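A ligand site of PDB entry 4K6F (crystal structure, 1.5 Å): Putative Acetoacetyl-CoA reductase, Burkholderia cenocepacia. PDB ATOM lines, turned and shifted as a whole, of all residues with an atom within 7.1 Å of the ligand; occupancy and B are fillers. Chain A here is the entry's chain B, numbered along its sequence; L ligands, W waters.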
ATOM      1  N   THR A  17       0.956 -13.934 -13.864  1.00  0.00           N
ATOM      2  CA  THR A  17       0.960 -15.345 -13.518  1.00  0.00           C
ATOM      3  C   THR A  17       2.333 -15.947 -13.794  1.00  0.00           C
ATOM      4  O   THR A  17       3.046 -15.547 -14.705  1.00  0.00           O
ATOM      5  CB  THR A  17      -0.150 -16.162 -14.216  1.00  0.00           C
ATOM      6  OG1 THR A  17       0.055 -16.169 -15.618  1.00  0.00           O
ATOM      7  CG2 THR A  17      -1.552 -15.626 -13.924  1.00  0.00           C
ATOM      8  N   GLY A  18       2.753 -16.901 -12.975  1.00  0.00           N
ATOM      9  CA  GLY A  18       4.147 -17.375 -13.056  1.00  0.00           C
ATOM     10  C   GLY A  18       5.139 -16.251 -12.784  1.00  0.00           C
ATOM     11  O   GLY A  18       6.229 -16.238 -13.360  1.00  0.00           O
ATOM     12  N   GLY A  19       4.751 -15.318 -11.918  1.00  0.00           N
ATOM     13  CA  GLY A  19       5.508 -14.077 -11.706  1.00  0.00           C
ATOM     14  C   GLY A  19       6.811 -14.190 -10.936  1.00  0.00           C
ATOM     15  O   GLY A  19       7.565 -13.226 -10.881  1.00  0.00           O
ATOM     16  N   MET A  20       7.101 -15.345 -10.342  1.00  0.00           N
ATOM     17  CA  MET A  20       8.249 -15.461  -9.430  1.00  0.00           C
ATOM     18  C   MET A  20       9.541 -16.018  -9.997  1.00  0.00           C
ATOM     19  O   MET A  20      10.563 -15.981  -9.311  1.00  0.00           O
ATOM     20  CB  MET A  20       7.874 -16.350  -8.242  1.00  0.00           C
ATOM     21  CG  MET A  20       6.861 -15.742  -7.309  1.00  0.00           C
ATOM     22  SD  MET A  20       6.851 -16.651  -5.755  1.00  0.00           S
ATOM     23  CE  MET A  20       5.539 -15.806  -4.869  1.00  0.00           C
ATOM     24  N   GLY A  21       9.516 -16.575 -11.198  1.00  0.00           N
ATOM     25  CA  GLY A  21      10.741 -17.120 -11.802  1.00  0.00           C
ATOM     26  C   GLY A  21      10.878 -16.674 -13.241  1.00  0.00           C
ATOM     27  O   GLY A  21       9.940 -16.115 -13.778  1.00  0.00           O
ATOM     28  N   GLY A  22      12.040 -16.920 -13.854  1.00  0.00           N
ATOM     29  CA  GLY A  22      12.264 -16.695 -15.279  1.00  0.00           C
ATOM     30  C   GLY A  22      11.705 -15.434 -15.904  1.00  0.00           C
ATOM     31  O   GLY A  22      11.918 -14.338 -15.399  1.00  0.00           O
ATOM     32  N   GLY A  24       8.586 -14.437 -16.095  1.00  0.00           N
ATOM     33  CA  GLY A  24       7.596 -13.821 -15.198  1.00  0.00           C
ATOM     34  C   GLY A  24       8.218 -12.844 -14.221  1.00  0.00           C
ATOM     35  O   GLY A  24       7.679 -11.751 -13.984  1.00  0.00           O
ATOM     36  N   GLU A  25       9.338 -13.227 -13.607  1.00  0.00           N
ATOM     37  CA  GLU A  25       9.990 -12.329 -12.638  1.00  0.00           C
ATOM     38  C   GLU A  25      10.456 -11.051 -13.318  1.00  0.00           C
ATOM     39  O   GLU A  25      10.346  -9.952 -12.760  1.00  0.00           O
ATOM     40  CB  GLU A  25      11.196 -12.999 -11.981  1.00  0.00           C
ATOM     41  CG  GLU A  25      11.931 -12.103 -11.001  1.00  0.00           C
ATOM     42  CD  GLU A  25      13.085 -12.794 -10.317  1.00  0.00           C
ATOM     43  OE1 GLU A  25      14.244 -12.413 -10.590  1.00  0.00           O
ATOM     44  OE2 GLU A  25      12.851 -13.720  -9.529  1.00  0.00           O
ATOM     45  N   THR A  41       1.232 -14.525  -9.134  1.00  0.00           N
ATOM     46  CA  THR A  41       0.736 -15.821  -8.702  1.00  0.00           C
ATOM     47  C   THR A  41       1.889 -16.829  -8.712  1.00  0.00           C
ATOM     48  O   THR A  41       2.878 -16.675  -9.456  1.00  0.00           O
ATOM     49  CB  THR A  41      -0.431 -16.360  -9.547  1.00  0.00           C
ATOM     50  OG1 THR A  41       0.029 -16.764 -10.844  1.00  0.00           O
ATOM     51  CG2 THR A  41      -1.550 -15.335  -9.658  1.00  0.00           C
ATOM     52  N   TYR A  42       1.738 -17.832  -7.865  1.00  0.00           N
ATOM     53  CA  TYR A  42       2.662 -18.962  -7.808  1.00  0.00           C
ATOM     54  C   TYR A  42       1.865 -20.255  -7.698  1.00  0.00           C
ATOM     55  O   TYR A  42       0.767 -20.261  -7.148  1.00  0.00           O
ATOM     56  CB  TYR A  42       3.658 -18.828  -6.659  1.00  0.00           C
ATOM     57  CG  TYR A  42       3.063 -18.788  -5.282  1.00  0.00           C
ATOM     58  CD1 TYR A  42       2.911 -19.959  -4.516  1.00  0.00           C
ATOM     59  CD2 TYR A  42       2.694 -17.575  -4.701  1.00  0.00           C
ATOM     60  CE1 TYR A  42       2.379 -19.917  -3.243  1.00  0.00           C
ATOM     61  CE2 TYR A  42       2.171 -17.529  -3.422  1.00  0.00           C
ATOM     62  CZ  TYR A  42       2.011 -18.699  -2.699  1.00  0.00           C
ATOM     63  OH  TYR A  42       1.499 -18.645  -1.422  1.00  0.00           O
ATOM     64  N   SER A  43       2.413 -21.335  -8.249  1.00  0.00           N
ATOM     65  CA  SER A  43       1.753 -22.625  -8.221  1.00  0.00           C
ATOM     66  C   SER A  43       1.638 -23.149  -6.778  1.00  0.00           C
ATOM     67  O   SER A  43       2.515 -22.878  -5.946  1.00  0.00           O
ATOM     68  CB  SER A  43       2.536 -23.623  -9.073  1.00  0.00           C
ATOM     69  OG  SER A  43       3.822 -23.857  -8.505  1.00  0.00           O
ATOM     70  N   PRO A  44       0.577 -23.936  -6.497  1.00  0.00           N
ATOM     71  CA  PRO A  44       0.229 -24.215  -5.106  1.00  0.00           C
ATOM     72  C   PRO A  44       1.311 -24.907  -4.306  1.00  0.00           C
ATOM     73  O   PRO A  44       1.359 -24.751  -3.102  1.00  0.00           O
ATOM     74  CB  PRO A  44      -1.026 -25.087  -5.219  1.00  0.00           C
ATOM     75  CG  PRO A  44      -1.604 -24.755  -6.561  1.00  0.00           C
ATOM     76  CD  PRO A  44      -0.381 -24.581  -7.422  1.00  0.00           C
ATOM     77  N   ASN A  45       2.193 -25.657  -4.966  1.00  0.00           N
ATOM     78  CA  ASN A  45       3.248 -26.381  -4.273  1.00  0.00           C
ATOM     79  C   ASN A  45       4.623 -25.747  -4.444  1.00  0.00           C
ATOM     80  O   ASN A  45       5.658 -26.390  -4.245  1.00  0.00           O
ATOM     81  CB  ASN A  45       3.210 -27.849  -4.678  1.00  0.00           C
ATOM     82  CG  ASN A  45       1.864 -28.479  -4.339  1.00  0.00           C
ATOM     83  OD1 ASN A  45       1.476 -28.545  -3.179  1.00  0.00           O
ATOM     84  ND2 ASN A  45       1.152 -28.950  -5.362  1.00  0.00           N
ATOM     85  N   ASN A  46       4.623 -24.457  -4.777  1.00  0.00           N
ATOM     86  CA  ASN A  46       5.852 -23.683  -4.795  1.00  0.00           C
ATOM     87  C   ASN A  46       6.180 -23.310  -3.351  1.00  0.00           C
ATOM     88  O   ASN A  46       5.431 -22.564  -2.713  1.00  0.00           O
ATOM     89  CB  ASN A  46       5.687 -22.434  -5.652  1.00  0.00           C
ATOM     90  CG  ASN A  46       6.976 -21.654  -5.788  1.00  0.00           C
ATOM     91  OD1 ASN A  46       7.882 -21.755  -4.954  1.00  0.00           O
ATOM     92  ND2 ASN A  46       7.072 -20.852  -6.838  1.00  0.00           N
ATOM     93  N   PRO A  67      -1.252 -18.038  -4.149  1.00  0.00           N
ATOM     94  CA  PRO A  67      -1.204 -19.336  -4.815  1.00  0.00           C
ATOM     95  C   PRO A  67      -2.384 -19.507  -5.767  1.00  0.00           C
ATOM     96  O   PRO A  67      -3.487 -19.085  -5.465  1.00  0.00           O
ATOM     97  CB  PRO A  67      -1.342 -20.335  -3.657  1.00  0.00           C
ATOM     98  CG  PRO A  67      -2.082 -19.598  -2.610  1.00  0.00           C
ATOM     99  CD  PRO A  67      -1.759 -18.129  -2.780  1.00  0.00           C
ATOM    100  N   VAL A  68      -2.131 -20.120  -6.921  1.00  0.00           N
ATOM    101  CA  VAL A  68      -3.217 -20.482  -7.831  1.00  0.00           C
ATOM    102  C   VAL A  68      -2.791 -21.684  -8.649  1.00  0.00           C
ATOM    103  O   VAL A  68      -1.618 -21.891  -8.896  1.00  0.00           O
ATOM    104  CB  VAL A  68      -3.598 -19.303  -8.765  1.00  0.00           C
ATOM    105  CG1 VAL A  68      -2.547 -19.127  -9.845  1.00  0.00           C
ATOM    106  CG2 VAL A  68      -4.978 -19.512  -9.379  1.00  0.00           C
ATOM    107  N   ASP A  69      -3.763 -22.510  -9.027  1.00  0.00           N
ATOM    108  CA  ASP A  69      -3.570 -23.500 -10.075  1.00  0.00           C
ATOM    109  C   ASP A  69      -4.250 -22.939 -11.308  1.00  0.00           C
ATOM    110  O   ASP A  69      -5.493 -22.965 -11.406  1.00  0.00           O
ATOM    111  CB  ASP A  69      -4.195 -24.838  -9.657  1.00  0.00           C
ATOM    112  CG  ASP A  69      -4.137 -25.895 -10.754  1.00  0.00           C
ATOM    113  OD1 ASP A  69      -3.507 -25.648 -11.816  1.00  0.00           O
ATOM    114  OD2 ASP A  69      -4.712 -26.980 -10.548  1.00  0.00           O
ATOM    115  N   VAL A  70      -3.465 -22.454 -12.268  1.00  0.00           N
ATOM    116  CA  VAL A  70      -4.062 -21.815 -13.439  1.00  0.00           C
ATOM    117  C   VAL A  70      -4.873 -22.779 -14.304  1.00  0.00           C
ATOM    118  O   VAL A  70      -5.700 -22.343 -15.077  1.00  0.00           O
ATOM    119  CB  VAL A  70      -3.072 -20.992 -14.301  1.00  0.00           C
ATOM    120  CG1 VAL A  70      -2.435 -19.887 -13.489  1.00  0.00           C
ATOM    121  CG2 VAL A  70      -2.015 -21.883 -14.962  1.00  0.00           C
ATOM    122  N   ALA A  71      -4.652 -24.090 -14.156  1.00  0.00           N
ATOM    123  CA  ALA A  71      -5.468 -25.070 -14.886  1.00  0.00           C
ATOM    124  C   ALA A  71      -6.876 -25.271 -14.285  1.00  0.00           C
ATOM    125  O   ALA A  71      -7.733 -25.889 -14.907  1.00  0.00           O
ATOM    126  CB  ALA A  71      -4.714 -26.382 -14.989  1.00  0.00           C
ATOM    127  N   ASP A  72      -7.113 -24.719 -13.091  1.00  0.00           N
ATOM    128  CA  ASP A  72      -8.343 -24.952 -12.335  1.00  0.00           C
ATOM    129  C   ASP A  72      -9.208 -23.680 -12.358  1.00  0.00           C
ATOM    130  O   ASP A  72      -8.818 -22.659 -11.800  1.00  0.00           O
ATOM    131  CB  ASP A  72      -7.947 -25.319 -10.904  1.00  0.00           C
ATOM    132  CG  ASP A  72      -9.130 -25.711 -10.021  1.00  0.00           C
ATOM    133  OD1 ASP A  72     -10.165 -25.012  -9.984  1.00  0.00           O
ATOM    134  OD2 ASP A  72      -8.980 -26.728  -9.314  1.00  0.00           O
ATOM    135  N   ASN A  96       1.269 -15.448 -18.251  1.00  0.00           N
ATOM    136  CA  ASN A  96       2.632 -15.908 -18.487  1.00  0.00           C
ATOM    137  C   ASN A  96       2.884 -17.342 -18.067  1.00  0.00           C
ATOM    138  O   ASN A  96       3.789 -18.006 -18.604  1.00  0.00           O
ATOM    139  CB  ASN A  96       3.620 -14.952 -17.789  1.00  0.00           C
ATOM    140  CG  ASN A  96       5.041 -15.498 -17.737  1.00  0.00           C
ATOM    141  OD1 ASN A  96       5.734 -15.494 -18.744  1.00  0.00           O
ATOM    142  ND2 ASN A  96       5.450 -16.015 -16.572  1.00  0.00           N
ATOM    143  N   ALA A  97       2.080 -17.842 -17.128  1.00  0.00           N
ATOM    144  CA  ALA A  97       2.234 -19.224 -16.686  1.00  0.00           C
ATOM    145  C   ALA A  97       2.099 -20.202 -17.868  1.00  0.00           C
ATOM    146  O   ALA A  97       1.239 -20.035 -18.723  1.00  0.00           O
ATOM    147  CB  ALA A  97       1.218 -19.567 -15.614  1.00  0.00           C
ATOM    148  N   GLY A  98       2.956 -21.217 -17.875  1.00  0.00           N
ATOM    149  CA  GLY A  98       2.955 -22.238 -18.889  1.00  0.00           C
ATOM    150  C   GLY A  98       4.022 -23.294 -18.623  1.00  0.00           C
ATOM    151  O   GLY A  98       5.001 -23.027 -17.910  1.00  0.00           O
ATOM    152  N   ILE A  99       3.849 -24.461 -19.221  1.00  0.00           N
ATOM    153  CA  ILE A  99       4.805 -25.562 -19.099  1.00  0.00           C
ATOM    154  C   ILE A  99       5.087 -26.170 -20.467  1.00  0.00           C
ATOM    155  O   ILE A  99       4.347 -25.925 -21.449  1.00  0.00           O
ATOM    156  CB  ILE A  99       4.300 -26.676 -18.141  1.00  0.00           C
ATOM    157  CG1 ILE A  99       3.025 -27.359 -18.674  1.00  0.00           C
ATOM    158  CG2 ILE A  99       4.052 -26.118 -16.728  1.00  0.00           C
ATOM    159  CD1 ILE A  99       2.493 -28.508 -17.840  1.00  0.00           C
ATOM    160  N   ARG A 101       5.885 -30.097 -22.067  1.00  0.00           N
ATOM    161  CA  ARG A 101       5.982 -31.562 -21.910  1.00  0.00           C
ATOM    162  C   ARG A 101       6.206 -32.136 -23.320  1.00  0.00           C
ATOM    163  O   ARG A 101       5.282 -32.743 -23.925  1.00  0.00           O
ATOM    164  CB  ARG A 101       4.722 -32.147 -21.274  1.00  0.00           C
ATOM    165  CG  ARG A 101       4.417 -31.651 -19.842  1.00  0.00           C
ATOM    166  CD  ARG A 101       5.382 -32.222 -18.782  1.00  0.00           C
ATOM    167  NE  ARG A 101       5.122 -31.716 -17.416  1.00  0.00           N
ATOM    168  CZ  ARG A 101       5.741 -30.686 -16.823  1.00  0.00           C
ATOM    169  NH1 ARG A 101       6.697 -29.987 -17.446  1.00  0.00           N
ATOM    170  NH2 ARG A 101       5.415 -30.318 -15.587  1.00  0.00           N
ATOM    171  N   ARG A 118      -4.297 -27.832 -20.796  1.00  0.00           N
ATOM    172  CA  ARG A 118      -4.963 -27.310 -19.600  1.00  0.00           C
ATOM    173  C   ARG A 118      -4.147 -26.189 -18.949  1.00  0.00           C
ATOM    174  O   ARG A 118      -4.700 -25.176 -18.536  1.00  0.00           O
ATOM    175  CB  ARG A 118      -5.221 -28.438 -18.589  1.00  0.00           C
ATOM    176  N   THR A 119      -2.838 -26.362 -18.856  1.00  0.00           N
ATOM    177  CA  THR A 119      -1.998 -25.397 -18.169  1.00  0.00           C
ATOM    178  C   THR A 119      -1.719 -24.147 -19.001  1.00  0.00           C
ATOM    179  O   THR A 119      -1.629 -23.034 -18.460  1.00  0.00           O
ATOM    180  CB  THR A 119      -0.659 -26.014 -17.732  1.00  0.00           C
ATOM    181  OG1 THR A 119      -0.941 -27.143 -16.913  1.00  0.00           O
ATOM    182  CG2 THR A 119       0.162 -25.056 -16.895  1.00  0.00           C
ATOM    183  N   ASN A 120      -1.606 -24.325 -20.311  1.00  0.00           N
ATOM    184  CA  ASN A 120      -1.139 -23.267 -21.209  1.00  0.00           C
ATOM    185  C   ASN A 120      -2.266 -22.528 -21.951  1.00  0.00           C
ATOM    186  O   ASN A 120      -2.104 -21.369 -22.325  1.00  0.00           O
ATOM    187  CB  ASN A 120      -0.138 -23.826 -22.233  1.00  0.00           C
ATOM    188  CG  ASN A 120       1.173 -24.288 -21.617  1.00  0.00           C
ATOM    189  OD1 ASN A 120       1.271 -24.511 -20.420  1.00  0.00           O
ATOM    190  ND2 ASN A 120       2.179 -24.447 -22.440  1.00  0.00           N
HETATM  191  C1  LIG L   1       6.994 -21.400 -15.735  1.00  0.00           C
HETATM  192  C2  LIG L   1       6.053 -20.618 -14.819  1.00  0.00           C
HETATM  193  O1  LIG L   1       4.705 -21.092 -14.944  1.00  0.00           O
HETATM  194  C3  LIG L   1       6.439 -20.726 -13.348  1.00  0.00           C
HETATM  195  O2  LIG L   1       6.642 -19.402 -12.843  1.00  0.00           O
HETATM  196  C4  LIG L   1       5.282 -21.470 -12.695  1.00  0.00           C
HETATM  197  O3  LIG L   1       4.907 -21.057 -11.377  1.00  0.00           O
HETATM  198  C5  LIG L   1       4.118 -21.199 -13.653  1.00  0.00           C
HETATM  199  N1  LIG L   1       3.138 -22.302 -13.656  1.00  0.00           N
HETATM  200  C6  LIG L   1       3.236 -23.437 -14.372  1.00  0.00           C
HETATM  201  N2  LIG L   1       2.163 -24.218 -14.146  1.00  0.00           N
HETATM  202  C7  LIG L   1       1.354 -23.591 -13.290  1.00  0.00           C
HETATM  203  C8  LIG L   1       0.064 -23.881 -12.636  1.00  0.00           C
HETATM  204  N3  LIG L   1      -0.573 -25.040 -12.903  1.00  0.00           N
HETATM  205  N4  LIG L   1      -0.452 -22.933 -11.792  1.00  0.00           N
HETATM  206  C9  LIG L   1       0.200 -21.783 -11.540  1.00  0.00           C
HETATM  207  N5  LIG L   1       1.389 -21.461 -12.106  1.00  0.00           N
HETATM  208  C10 LIG L   1       2.008 -22.309 -12.958  1.00  0.00           C
HETATM  209  P1  LIG L   1       5.769 -21.320 -10.049  1.00  0.00           P
HETATM  210  O4  LIG L   1       7.023 -20.480 -10.251  1.00  0.00           O
HETATM  211  O5  LIG L   1       5.991 -22.800 -10.037  1.00  0.00           O
HETATM  212  O6  LIG L   1       4.871 -20.836  -8.940  1.00  0.00           O
HETATM  213  O   HOH W   1       0.047 -27.517 -14.284  1.00  0.00           O
HETATM  214  O   HOH W   2       7.765 -24.358 -16.225  1.00  0.00           O
HETATM  215  O   HOH W   3       5.369 -17.755  -9.977  1.00  0.00           O
HETATM  216  O   HOH W   4       1.840 -18.842 -11.056  1.00  0.00           O
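Water W4 lies within hydrogen-bond range of OG1 of Thr 41 (2.8 Å), N5 of the ligand (2.9 Å), N of Gly 18 (2.9 Å) and N of Tyr 42 (3.3 Å). Water W1 lies within hydrogen-bond range of OG1 of Thr 119 (2.8 Å) and N3 of the ligand (2.9 Å). Water W3 lies within hydrogen-bond range of O of Thr 41 (2.8 Å), N of Met 20 (3.0 Å), N of Gly 19 (3.2 Å) and O4 of the ligand (3.2 Å).
O of Val 68 lies close to N4 of the ligand (3.3 Å). Tyr 42 touches the ligand (CA to O6, 3.1 Å). Ala 97 touches the ligand (CA to O1, 3.6 Å). Ile 99 touches the ligand (CG2 to C6, 3.7 Å). Thr 119 touches the ligand (CG2 to N2, 3.5 Å). Of the 28 residues printed, 11 come within 4 Å of the ligand. The nearest printed residue that does not touch the ligand is Gly 21 (4.4 Å).
The backbone NH (N) of Ser 43 is in hydrogen-bond range of an oxygen (O6) of the ligand, 2.6 Å away. An oxygen (O5) of the ligand is in hydrogen-bond range of the side-chain hydroxyl (OG) of Ser 43, at 2.9 Å. ND2 of Asn 46 sits at hydrogen-bond distance from O6 of the ligand (3.0 Å). N4 of the ligand lies within hydrogen-bond range of N of Val 70 (3.1 Å). The side-chain carboxylate of Asp 69 is in hydrogen-bond range of a nitrogen (N3) of the ligand. The backbone carbonyl oxygen (O) of Gly 18 lies close to an oxygen (O2) of the ligand, 3.2 Å away. The backbone NH (N) of Gly 98 is in hydrogen-bond range of an oxygen (O1) of the ligand (3.4 Å).
N of Val 68 is in hydrogen-bond range of O of Tyr 42 (2.9 Å). The side-chain carboxylate (OD1) of Asp 69 lies within hydrogen-bond range of the backbone NH (N) of Ala 71, at 3.0 Å. The side-chain hydroxyl of Thr 41 is in hydrogen-bond range of the backbone NH of Gly 18 (3.5 Å). The side-chain amide nitrogen (ND2) of Asn 96 sits at hydrogen-bond distance from the backbone carbonyl oxygen (O) of Gly 18 (3.3 Å). OG1 of Thr 17 is in hydrogen-bond range of N of Ala 97 (3.0 Å). O of Ile 99 lies within hydrogen-bond range of ND2 of Asn 120 (2.8 Å).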
